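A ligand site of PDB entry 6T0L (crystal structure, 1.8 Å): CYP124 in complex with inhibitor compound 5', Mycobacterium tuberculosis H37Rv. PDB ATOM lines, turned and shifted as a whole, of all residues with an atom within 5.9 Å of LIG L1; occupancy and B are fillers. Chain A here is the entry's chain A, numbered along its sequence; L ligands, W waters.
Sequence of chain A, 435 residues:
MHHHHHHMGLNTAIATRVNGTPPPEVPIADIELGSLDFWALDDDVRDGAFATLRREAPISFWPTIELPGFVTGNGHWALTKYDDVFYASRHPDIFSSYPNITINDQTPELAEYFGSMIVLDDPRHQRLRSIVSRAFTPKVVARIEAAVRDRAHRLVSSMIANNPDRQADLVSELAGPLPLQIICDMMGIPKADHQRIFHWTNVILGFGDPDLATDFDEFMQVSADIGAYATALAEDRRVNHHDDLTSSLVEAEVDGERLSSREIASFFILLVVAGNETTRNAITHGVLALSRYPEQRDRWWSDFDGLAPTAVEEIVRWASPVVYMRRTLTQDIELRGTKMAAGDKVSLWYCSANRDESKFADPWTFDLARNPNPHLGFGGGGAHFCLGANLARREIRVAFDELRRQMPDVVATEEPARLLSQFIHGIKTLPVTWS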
ATOM      1  N   ILE A 101      23.722 -20.386 -17.754  1.00  0.00           N
ATOM      2  CA  ILE A 101      24.928 -19.626 -17.452  1.00  0.00           C
ATOM      3  C   ILE A 101      24.724 -18.632 -16.304  1.00  0.00           C
ATOM      4  O   ILE A 101      25.635 -17.878 -15.962  1.00  0.00           O
ATOM      5  CB  ILE A 101      25.507 -18.937 -18.712  1.00  0.00           C
ATOM      6  CG1 ILE A 101      24.420 -18.228 -19.526  1.00  0.00           C
ATOM      7  CG2 ILE A 101      26.210 -20.011 -19.578  1.00  0.00           C
ATOM      8  CD1 ILE A 101      23.922 -16.919 -18.858  1.00  0.00           C
ATOM      9  N   THR A 102      23.549 -18.637 -15.660  1.00  0.00           N
ATOM     10  CA  THR A 102      23.489 -18.073 -14.325  1.00  0.00           C
ATOM     11  C   THR A 102      23.451 -19.231 -13.332  1.00  0.00           C
ATOM     12  O   THR A 102      23.225 -20.392 -13.695  1.00  0.00           O
ATOM     13  CB  THR A 102      22.277 -17.133 -14.139  1.00  0.00           C
ATOM     14  OG1 THR A 102      21.071 -17.832 -14.443  1.00  0.00           O
ATOM     15  CG2 THR A 102      22.405 -15.848 -15.045  1.00  0.00           C
ATOM     16  N   PHE A 114      14.672 -18.568 -22.776  1.00  0.00           N
ATOM     17  CA  PHE A 114      16.085 -18.413 -22.429  1.00  0.00           C
ATOM     18  C   PHE A 114      16.903 -19.624 -22.839  1.00  0.00           C
ATOM     19  O   PHE A 114      17.760 -20.112 -22.081  1.00  0.00           O
ATOM     20  CB  PHE A 114      16.232 -18.108 -20.944  1.00  0.00           C
ATOM     21  CG  PHE A 114      15.504 -16.856 -20.515  1.00  0.00           C
ATOM     22  CD1 PHE A 114      15.935 -15.612 -20.942  1.00  0.00           C
ATOM     23  CD2 PHE A 114      14.367 -16.919 -19.710  1.00  0.00           C
ATOM     24  CE1 PHE A 114      15.259 -14.445 -20.582  1.00  0.00           C
ATOM     25  CE2 PHE A 114      13.686 -15.768 -19.348  1.00  0.00           C
ATOM     26  CZ  PHE A 114      14.130 -14.525 -19.787  1.00  0.00           C
ATOM     27  N   SER A 116      18.942 -19.779 -25.714  1.00  0.00           N
ATOM     28  CA  SER A 116      19.749 -19.309 -26.836  1.00  0.00           C
ATOM     29  C   SER A 116      21.096 -20.058 -26.879  1.00  0.00           C
ATOM     30  O   SER A 116      21.394 -20.935 -26.063  1.00  0.00           O
ATOM     31  CB  SER A 116      19.995 -17.812 -26.736  1.00  0.00           C
ATOM     32  OG  SER A 116      20.931 -17.503 -25.692  1.00  0.00           O
ATOM     33  N   ILE A 118      23.877 -19.159 -25.937  1.00  0.00           N
ATOM     34  CA  ILE A 118      24.776 -18.930 -24.821  1.00  0.00           C
ATOM     35  C   ILE A 118      24.644 -20.028 -23.770  1.00  0.00           C
ATOM     36  O   ILE A 118      25.552 -20.179 -22.936  1.00  0.00           O
ATOM     37  CB  ILE A 118      24.575 -17.534 -24.183  1.00  0.00           C
ATOM     38  CG1 ILE A 118      25.832 -17.124 -23.423  1.00  0.00           C
ATOM     39  CG2 ILE A 118      23.329 -17.504 -23.235  1.00  0.00           C
ATOM     40  CD1 ILE A 118      25.771 -15.744 -22.753  1.00  0.00           C
ATOM     41  N   ILE A 204      14.266  -8.147 -16.626  1.00  0.00           N
ATOM     42  CA  ILE A 204      14.918  -9.456 -16.788  1.00  0.00           C
ATOM     43  C   ILE A 204      16.262  -9.471 -16.098  1.00  0.00           C
ATOM     44  O   ILE A 204      16.601 -10.441 -15.390  1.00  0.00           O
ATOM     45  CB  ILE A 204      15.027  -9.813 -18.285  1.00  0.00           C
ATOM     46  CG1 ILE A 204      13.667 -10.242 -18.826  1.00  0.00           C
ATOM     47  CG2 ILE A 204      16.049 -10.938 -18.485  1.00  0.00           C
ATOM     48  CD1 ILE A 204      13.593 -10.226 -20.346  1.00  0.00           C
ATOM     49  N   LEU A 205      17.028  -8.390 -16.179  1.00  0.00           N
ATOM     50  CA  LEU A 205      18.349  -8.384 -15.523  1.00  0.00           C
ATOM     51  C   LEU A 205      18.380  -7.688 -14.178  1.00  0.00           C
ATOM     52  O   LEU A 205      19.452  -7.604 -13.552  1.00  0.00           O
ATOM     53  CB  LEU A 205      19.390  -7.733 -16.431  1.00  0.00           C
ATOM     54  CG  LEU A 205      19.707  -8.419 -17.759  1.00  0.00           C
ATOM     55  CD1 LEU A 205      20.786  -7.608 -18.458  1.00  0.00           C
ATOM     56  CD2 LEU A 205      20.175  -9.839 -17.533  1.00  0.00           C
ATOM     57  N   ILE A 269      15.808 -12.328 -27.837  1.00  0.00           N
ATOM     58  CA  ILE A 269      15.950 -11.863 -26.470  1.00  0.00           C
ATOM     59  C   ILE A 269      17.421 -11.773 -26.069  1.00  0.00           C
ATOM     60  O   ILE A 269      17.841 -10.796 -25.435  1.00  0.00           O
ATOM     61  CB  ILE A 269      15.143 -12.787 -25.545  1.00  0.00           C
ATOM     62  CG1 ILE A 269      13.636 -12.567 -25.803  1.00  0.00           C
ATOM     63  CG2 ILE A 269      15.524 -12.527 -24.079  1.00  0.00           C
ATOM     64  CD1 ILE A 269      12.729 -13.640 -25.135  1.00  0.00           C
ATOM     65  N   LEU A 270      18.234 -12.782 -26.427  1.00  0.00           N
ATOM     66  CA  LEU A 270      19.656 -12.728 -26.111  1.00  0.00           C
ATOM     67  C   LEU A 270      20.296 -11.485 -26.703  1.00  0.00           C
ATOM     68  O   LEU A 270      20.993 -10.738 -26.007  1.00  0.00           O
ATOM     69  CB  LEU A 270      20.380 -13.967 -26.613  1.00  0.00           C
ATOM     70  CG  LEU A 270      21.897 -13.854 -26.687  1.00  0.00           C
ATOM     71  CD1 LEU A 270      22.557 -13.817 -25.258  1.00  0.00           C
ATOM     72  CD2 LEU A 270      22.457 -15.027 -27.443  1.00  0.00           C
ATOM     73  N   VAL A 273      18.970  -8.075 -25.048  1.00  0.00           N
ATOM     74  CA  VAL A 273      19.395  -7.865 -23.679  1.00  0.00           C
ATOM     75  C   VAL A 273      20.912  -7.690 -23.619  1.00  0.00           C
ATOM     76  O   VAL A 273      21.414  -6.760 -22.990  1.00  0.00           O
ATOM     77  CB  VAL A 273      18.894  -9.002 -22.786  1.00  0.00           C
ATOM     78  CG1 VAL A 273      19.603  -8.933 -21.466  1.00  0.00           C
ATOM     79  CG2 VAL A 273      17.360  -8.876 -22.605  1.00  0.00           C
ATOM     80  N   ALA A 274      21.666  -8.561 -24.321  1.00  0.00           N
ATOM     81  CA  ALA A 274      23.117  -8.439 -24.333  1.00  0.00           C
ATOM     82  C   ALA A 274      23.550  -7.113 -24.953  1.00  0.00           C
ATOM     83  O   ALA A 274      24.577  -6.559 -24.552  1.00  0.00           O
ATOM     84  CB  ALA A 274      23.757  -9.587 -25.112  1.00  0.00           C
ATOM     85  N   GLY A 275      22.767  -6.593 -25.912  1.00  0.00           N
ATOM     86  CA  GLY A 275      23.230  -5.408 -26.608  1.00  0.00           C
ATOM     87  C   GLY A 275      23.027  -4.089 -25.921  1.00  0.00           C
ATOM     88  O   GLY A 275      23.509  -3.074 -26.425  1.00  0.00           O
ATOM     89  N   ASN A 276      22.324  -4.032 -24.804  1.00  0.00           N
ATOM     90  CA  ASN A 276      22.271  -2.678 -24.261  1.00  0.00           C
ATOM     91  C   ASN A 276      22.695  -2.573 -22.789  1.00  0.00           C
ATOM     92  O   ASN A 276      23.380  -1.605 -22.440  1.00  0.00           O
ATOM     93  CB  ASN A 276      20.862  -2.058 -24.479  1.00  0.00           C
ATOM     94  CG  ASN A 276      19.797  -2.618 -23.556  1.00  0.00           C
ATOM     95  OD1 ASN A 276      19.485  -2.023 -22.526  1.00  0.00           O
ATOM     96  ND2 ASN A 276      19.198  -3.746 -23.947  1.00  0.00           N
ATOM     97  N   GLU A 277      22.379  -3.545 -21.938  1.00  0.00           N
ATOM     98  CA  GLU A 277      22.566  -3.325 -20.511  1.00  0.00           C
ATOM     99  C   GLU A 277      24.041  -3.192 -20.098  1.00  0.00           C
ATOM    100  O   GLU A 277      24.399  -2.285 -19.319  1.00  0.00           O
ATOM    101  CB  GLU A 277      21.868  -4.457 -19.745  1.00  0.00           C
ATOM    102  CG  GLU A 277      21.336  -4.003 -18.433  1.00  0.00           C
ATOM    103  CD  GLU A 277      22.370  -4.197 -17.353  1.00  0.00           C
ATOM    104  OE1 GLU A 277      23.406  -4.823 -17.673  1.00  0.00           O
ATOM    105  OE2 GLU A 277      22.132  -3.742 -16.208  1.00  0.00           O
ATOM    106  N   THR A 278      24.926  -4.075 -20.584  1.00  0.00           N
ATOM    107  CA  THR A 278      26.314  -4.039 -20.084  1.00  0.00           C
ATOM    108  C   THR A 278      27.040  -2.785 -20.559  1.00  0.00           C
ATOM    109  O   THR A 278      27.893  -2.248 -19.844  1.00  0.00           O
ATOM    110  CB  THR A 278      27.092  -5.269 -20.536  1.00  0.00           C
ATOM    111  OG1 THR A 278      26.841  -5.474 -21.931  1.00  0.00           O
ATOM    112  CG2 THR A 278      26.670  -6.506 -19.778  1.00  0.00           C
ATOM    113  N   THR A 279      26.797  -2.356 -21.808  1.00  0.00           N
ATOM    114  CA  THR A 279      27.439  -1.137 -22.288  1.00  0.00           C
ATOM    115  C   THR A 279      26.980   0.062 -21.476  1.00  0.00           C
ATOM    116  O   THR A 279      27.778   0.980 -21.191  1.00  0.00           O
ATOM    117  CB  THR A 279      27.115  -0.945 -23.775  1.00  0.00           C
ATOM    118  OG1 THR A 279      27.640  -2.064 -24.501  1.00  0.00           O
ATOM    119  CG2 THR A 279      27.761   0.314 -24.301  1.00  0.00           C
ATOM    120  N   VAL A 322      29.674  -7.521 -16.315  1.00  0.00           N
ATOM    121  CA  VAL A 322      29.201  -8.868 -16.000  1.00  0.00           C
ATOM    122  C   VAL A 322      30.068  -9.373 -14.866  1.00  0.00           C
ATOM    123  O   VAL A 322      31.292  -9.511 -15.032  1.00  0.00           O
ATOM    124  CB  VAL A 322      29.283  -9.820 -17.213  1.00  0.00           C
ATOM    125  CG1 VAL A 322      28.756 -11.230 -16.827  1.00  0.00           C
ATOM    126  CG2 VAL A 322      28.458  -9.276 -18.361  1.00  0.00           C
ATOM    127  N   MET A 325      29.857 -15.501 -14.966  1.00  0.00           N
ATOM    128  CA  MET A 325      29.049 -16.449 -15.720  1.00  0.00           C
ATOM    129  C   MET A 325      29.272 -17.854 -15.139  1.00  0.00           C
ATOM    130  O   MET A 325      30.338 -18.157 -14.617  1.00  0.00           O
ATOM    131  CB  MET A 325      29.396 -16.488 -17.202  1.00  0.00           C
ATOM    132  CG  MET A 325      28.951 -15.203 -17.944  1.00  0.00           C
ATOM    133  SD  MET A 325      27.280 -15.392 -18.551  1.00  0.00           S
ATOM    134  CE  MET A 325      27.087 -13.785 -19.434  1.00  0.00           C
ATOM    135  N   CYS A 386      32.503 -12.642 -26.104  1.00  0.00           N
ATOM    136  CA  CYS A 386      31.418 -11.684 -26.343  1.00  0.00           C
ATOM    137  C   CYS A 386      31.271 -11.329 -27.827  1.00  0.00           C
ATOM    138  O   CYS A 386      32.202 -10.799 -28.445  1.00  0.00           O
ATOM    139  CB  CYS A 386      31.682 -10.398 -25.552  1.00  0.00           C
ATOM    140  SG  CYS A 386      30.377  -9.138 -25.895  1.00  0.00           S
ATOM    141  N   PHE A 423      24.917 -10.735 -10.441  1.00  0.00           N
ATOM    142  CA  PHE A 423      25.241 -11.087 -11.817  1.00  0.00           C
ATOM    143  C   PHE A 423      25.706  -9.881 -12.639  1.00  0.00           C
ATOM    144  O   PHE A 423      26.632 -10.007 -13.448  1.00  0.00           O
ATOM    145  CB  PHE A 423      23.996 -11.712 -12.443  1.00  0.00           C
ATOM    146  CG  PHE A 423      24.124 -12.185 -13.867  1.00  0.00           C
ATOM    147  CD1 PHE A 423      25.231 -12.899 -14.303  1.00  0.00           C
ATOM    148  CD2 PHE A 423      23.079 -11.959 -14.747  1.00  0.00           C
ATOM    149  CE1 PHE A 423      25.317 -13.354 -15.637  1.00  0.00           C
ATOM    150  CE2 PHE A 423      23.126 -12.400 -16.072  1.00  0.00           C
ATOM    151  CZ  PHE A 423      24.255 -13.110 -16.519  1.00  0.00           C
ATOM    152  N   ILE A 424      25.137  -8.704 -12.368  1.00  0.00           N
ATOM    153  CA  ILE A 424      25.310  -7.475 -13.157  1.00  0.00           C
ATOM    154  C   ILE A 424      25.825  -6.376 -12.246  1.00  0.00           C
ATOM    155  O   ILE A 424      25.235  -6.131 -11.180  1.00  0.00           O
ATOM    156  CB  ILE A 424      23.959  -7.046 -13.784  1.00  0.00           C
ATOM    157  CG1 ILE A 424      23.409  -8.134 -14.700  1.00  0.00           C
ATOM    158  CG2 ILE A 424      24.076  -5.666 -14.491  1.00  0.00           C
ATOM    159  CD1 ILE A 424      24.310  -8.447 -15.880  1.00  0.00           C
HETATM  160  C1  LIG L   1      22.740 -13.077 -20.470  1.00  0.00           C
HETATM  161  C2  LIG L   1      20.372 -13.673 -19.777  1.00  0.00           C
HETATM  162  C3  LIG L   1      19.448 -13.725 -20.990  1.00  0.00           C
HETATM  163  C4  LIG L   1      20.172 -14.100 -22.267  1.00  0.00           C
HETATM  164  C5  LIG L   1      18.682 -12.425 -21.170  1.00  0.00           C
HETATM  165  C6  LIG L   1      23.453 -13.186 -21.660  1.00  0.00           C
HETATM  166  C7  LIG L   1      24.303 -12.183 -22.091  1.00  0.00           C
HETATM  167  C8  LIG L   1      24.487 -11.054 -21.324  1.00  0.00           C
HETATM  168  C9  LIG L   1      23.810 -10.908 -20.104  1.00  0.00           C
HETATM  169  C10 LIG L   1      22.939 -11.928 -19.704  1.00  0.00           C
HETATM  170  C11 LIG L   1      24.015  -9.695 -19.247  1.00  0.00           C
HETATM  171  C12 LIG L   1      26.379 -10.220 -22.658  1.00  0.00           C
HETATM  172  C13 LIG L   1      21.790 -14.163 -20.035  1.00  0.00           C
HETATM  173  N1  LIG L   1      25.403 -10.032 -21.735  1.00  0.00           N
HETATM  174  N2  LIG L   1      26.841  -9.235 -23.371  1.00  0.00           N
HETATM  175  O1  LIG L   1      26.216  -8.021 -22.966  1.00  0.00           O
HETATM  176  C1  LG2 L   2      28.723 -12.841 -24.307  1.00  0.00           C
HETATM  177  C2  LG2 L   2      30.362  -9.172 -21.639  1.00  0.00           C
HETATM  178  C3  LG2 L   2      28.570  -5.975 -24.846  1.00  0.00           C
HETATM  179  C4  LG2 L   2      26.438  -9.669 -27.196  1.00  0.00           C
HETATM  180  C5  LG2 L   2      29.351 -12.120 -23.329  1.00  0.00           C
HETATM  181  C6  LG2 L   2      30.028 -12.678 -22.161  1.00  0.00           C
HETATM  182  C7  LG2 L   2      30.466 -11.667 -21.442  1.00  0.00           C
HETATM  183  C8  LG2 L   2      30.078 -10.434 -22.088  1.00  0.00           C
HETATM  184  C9  LG2 L   2      31.255 -11.735 -20.118  1.00  0.00           C
HETATM  185  C10 LG2 L   2      30.197 -14.186 -21.882  1.00  0.00           C
HETATM  186  C11 LG2 L   2      31.536 -14.631 -22.488  1.00  0.00           C
HETATM  187  C12 LG2 L   2      31.907 -16.063 -22.163  1.00  0.00           C
HETATM  188  O1  LG2 L   2      33.084 -16.440 -22.444  1.00  0.00           O
HETATM  189  O2  LG2 L   2      31.021 -16.809 -21.673  1.00  0.00           O
HETATM  190  C13 LG2 L   2      30.021  -7.985 -22.276  1.00  0.00           C
HETATM  191  C14 LG2 L   2      30.426  -6.666 -21.834  1.00  0.00           C
HETATM  192  C15 LG2 L   2      29.930  -5.774 -22.726  1.00  0.00           C
HETATM  193  C16 LG2 L   2      29.195  -6.509 -23.743  1.00  0.00           C
HETATM  194  C17 LG2 L   2      31.255  -6.311 -20.558  1.00  0.00           C
HETATM  195  C18 LG2 L   2      30.047  -4.241 -22.706  1.00  0.00           C
HETATM  196  C19 LG2 L   2      31.009  -3.484 -22.149  1.00  0.00           C
HETATM  197  C20 LG2 L   2      27.856  -6.699 -25.755  1.00  0.00           C
HETATM  198  C21 LG2 L   2      27.113  -6.136 -26.850  1.00  0.00           C
HETATM  199  C22 LG2 L   2      26.497  -7.131 -27.499  1.00  0.00           C
HETATM  200  C23 LG2 L   2      26.830  -8.402 -26.827  1.00  0.00           C
HETATM  201  C24 LG2 L   2      27.092  -4.618 -27.207  1.00  0.00           C
HETATM  202  C25 LG2 L   2      25.624  -6.935 -28.786  1.00  0.00           C
HETATM  203  C26 LG2 L   2      24.579  -7.734 -29.000  1.00  0.00           C
HETATM  204  C27 LG2 L   2      26.876 -10.836 -26.607  1.00  0.00           C
HETATM  205  C28 LG2 L   2      26.443 -12.161 -26.995  1.00  0.00           C
HETATM  206  C29 LG2 L   2      27.073 -13.062 -26.179  1.00  0.00           C
HETATM  207  C30 LG2 L   2      27.923 -12.294 -25.285  1.00  0.00           C
HETATM  208  C31 LG2 L   2      25.429 -12.488 -28.115  1.00  0.00           C
HETATM  209  C32 LG2 L   2      26.937 -14.615 -26.244  1.00  0.00           C
HETATM  210  C33 LG2 L   2      28.034 -15.130 -27.187  1.00  0.00           C
HETATM  211  C34 LG2 L   2      28.057 -16.636 -27.344  1.00  0.00           C
HETATM  212  O3  LG2 L   2      28.747 -17.130 -28.275  1.00  0.00           O
HETATM  213  O4  LG2 L   2      27.393 -17.338 -26.531  1.00  0.00           O
HETATM  214  N1  LG2 L   2      29.377 -10.763 -23.218  1.00  0.00           N
HETATM  215  N2  LG2 L   2      29.295  -7.857 -23.456  1.00  0.00           N
HETATM  216  N3  LG2 L   2      27.641  -8.076 -25.781  1.00  0.00           N
HETATM  217  N4  LG2 L   2      27.771 -10.927 -25.560  1.00  0.00           N
HETATM  218 FE1  LG2 L   2      28.519  -9.342 -24.498  1.00  0.00          FE
HETATM  219  O   HOH W   1      24.039  -6.578 -21.689  1.00  0.00           O
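Residues that only touch LIG L1: Ile 101, Phe 114, Ile 118, Leu 205, Leu 270, Val 273, Phe 423 and Ile 424. Hydrophobic or aromatic side chains that line LIG L1: Ile 101, Phe 114, Ile 118, Leu 205, Leu 270, Val 273, Ala 274, Phe 423 and Ile 424. The nearest printed residue that does not touch LIG L1 is Ile 204 (4.04 Å).
FE1 of LG2 L2 is bound by N2 of LIG L1 (2.0 Å).
OG of Ser 116 lies close to N of Ile 118, 3.4 Å away.
The side-chain sulfur (SG) of Cys 386 binds an iron atom (FE1) of LG2 L2, at 2.3 Å. The side-chain hydroxyl of Thr 278 lies within hydrogen-bond range of an oxygen (O1) of LIG L1, at 2.8 Å. O of Ala 274 is in hydrogen-bond range of O1 of LIG L1.
Water W1 lies within hydrogen-bond range of the backbone NH (N) of Thr 278 (2.9 Å), an oxygen (O1) of LIG L1 (2.9 Å), the backbone carbonyl oxygen (O) of Ala 274 (2.9 Å), the backbone carbonyl oxygen (O) of Val 273 (2.9 Å) and the backbone NH (N) of Glu 277 (3.5 Å).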
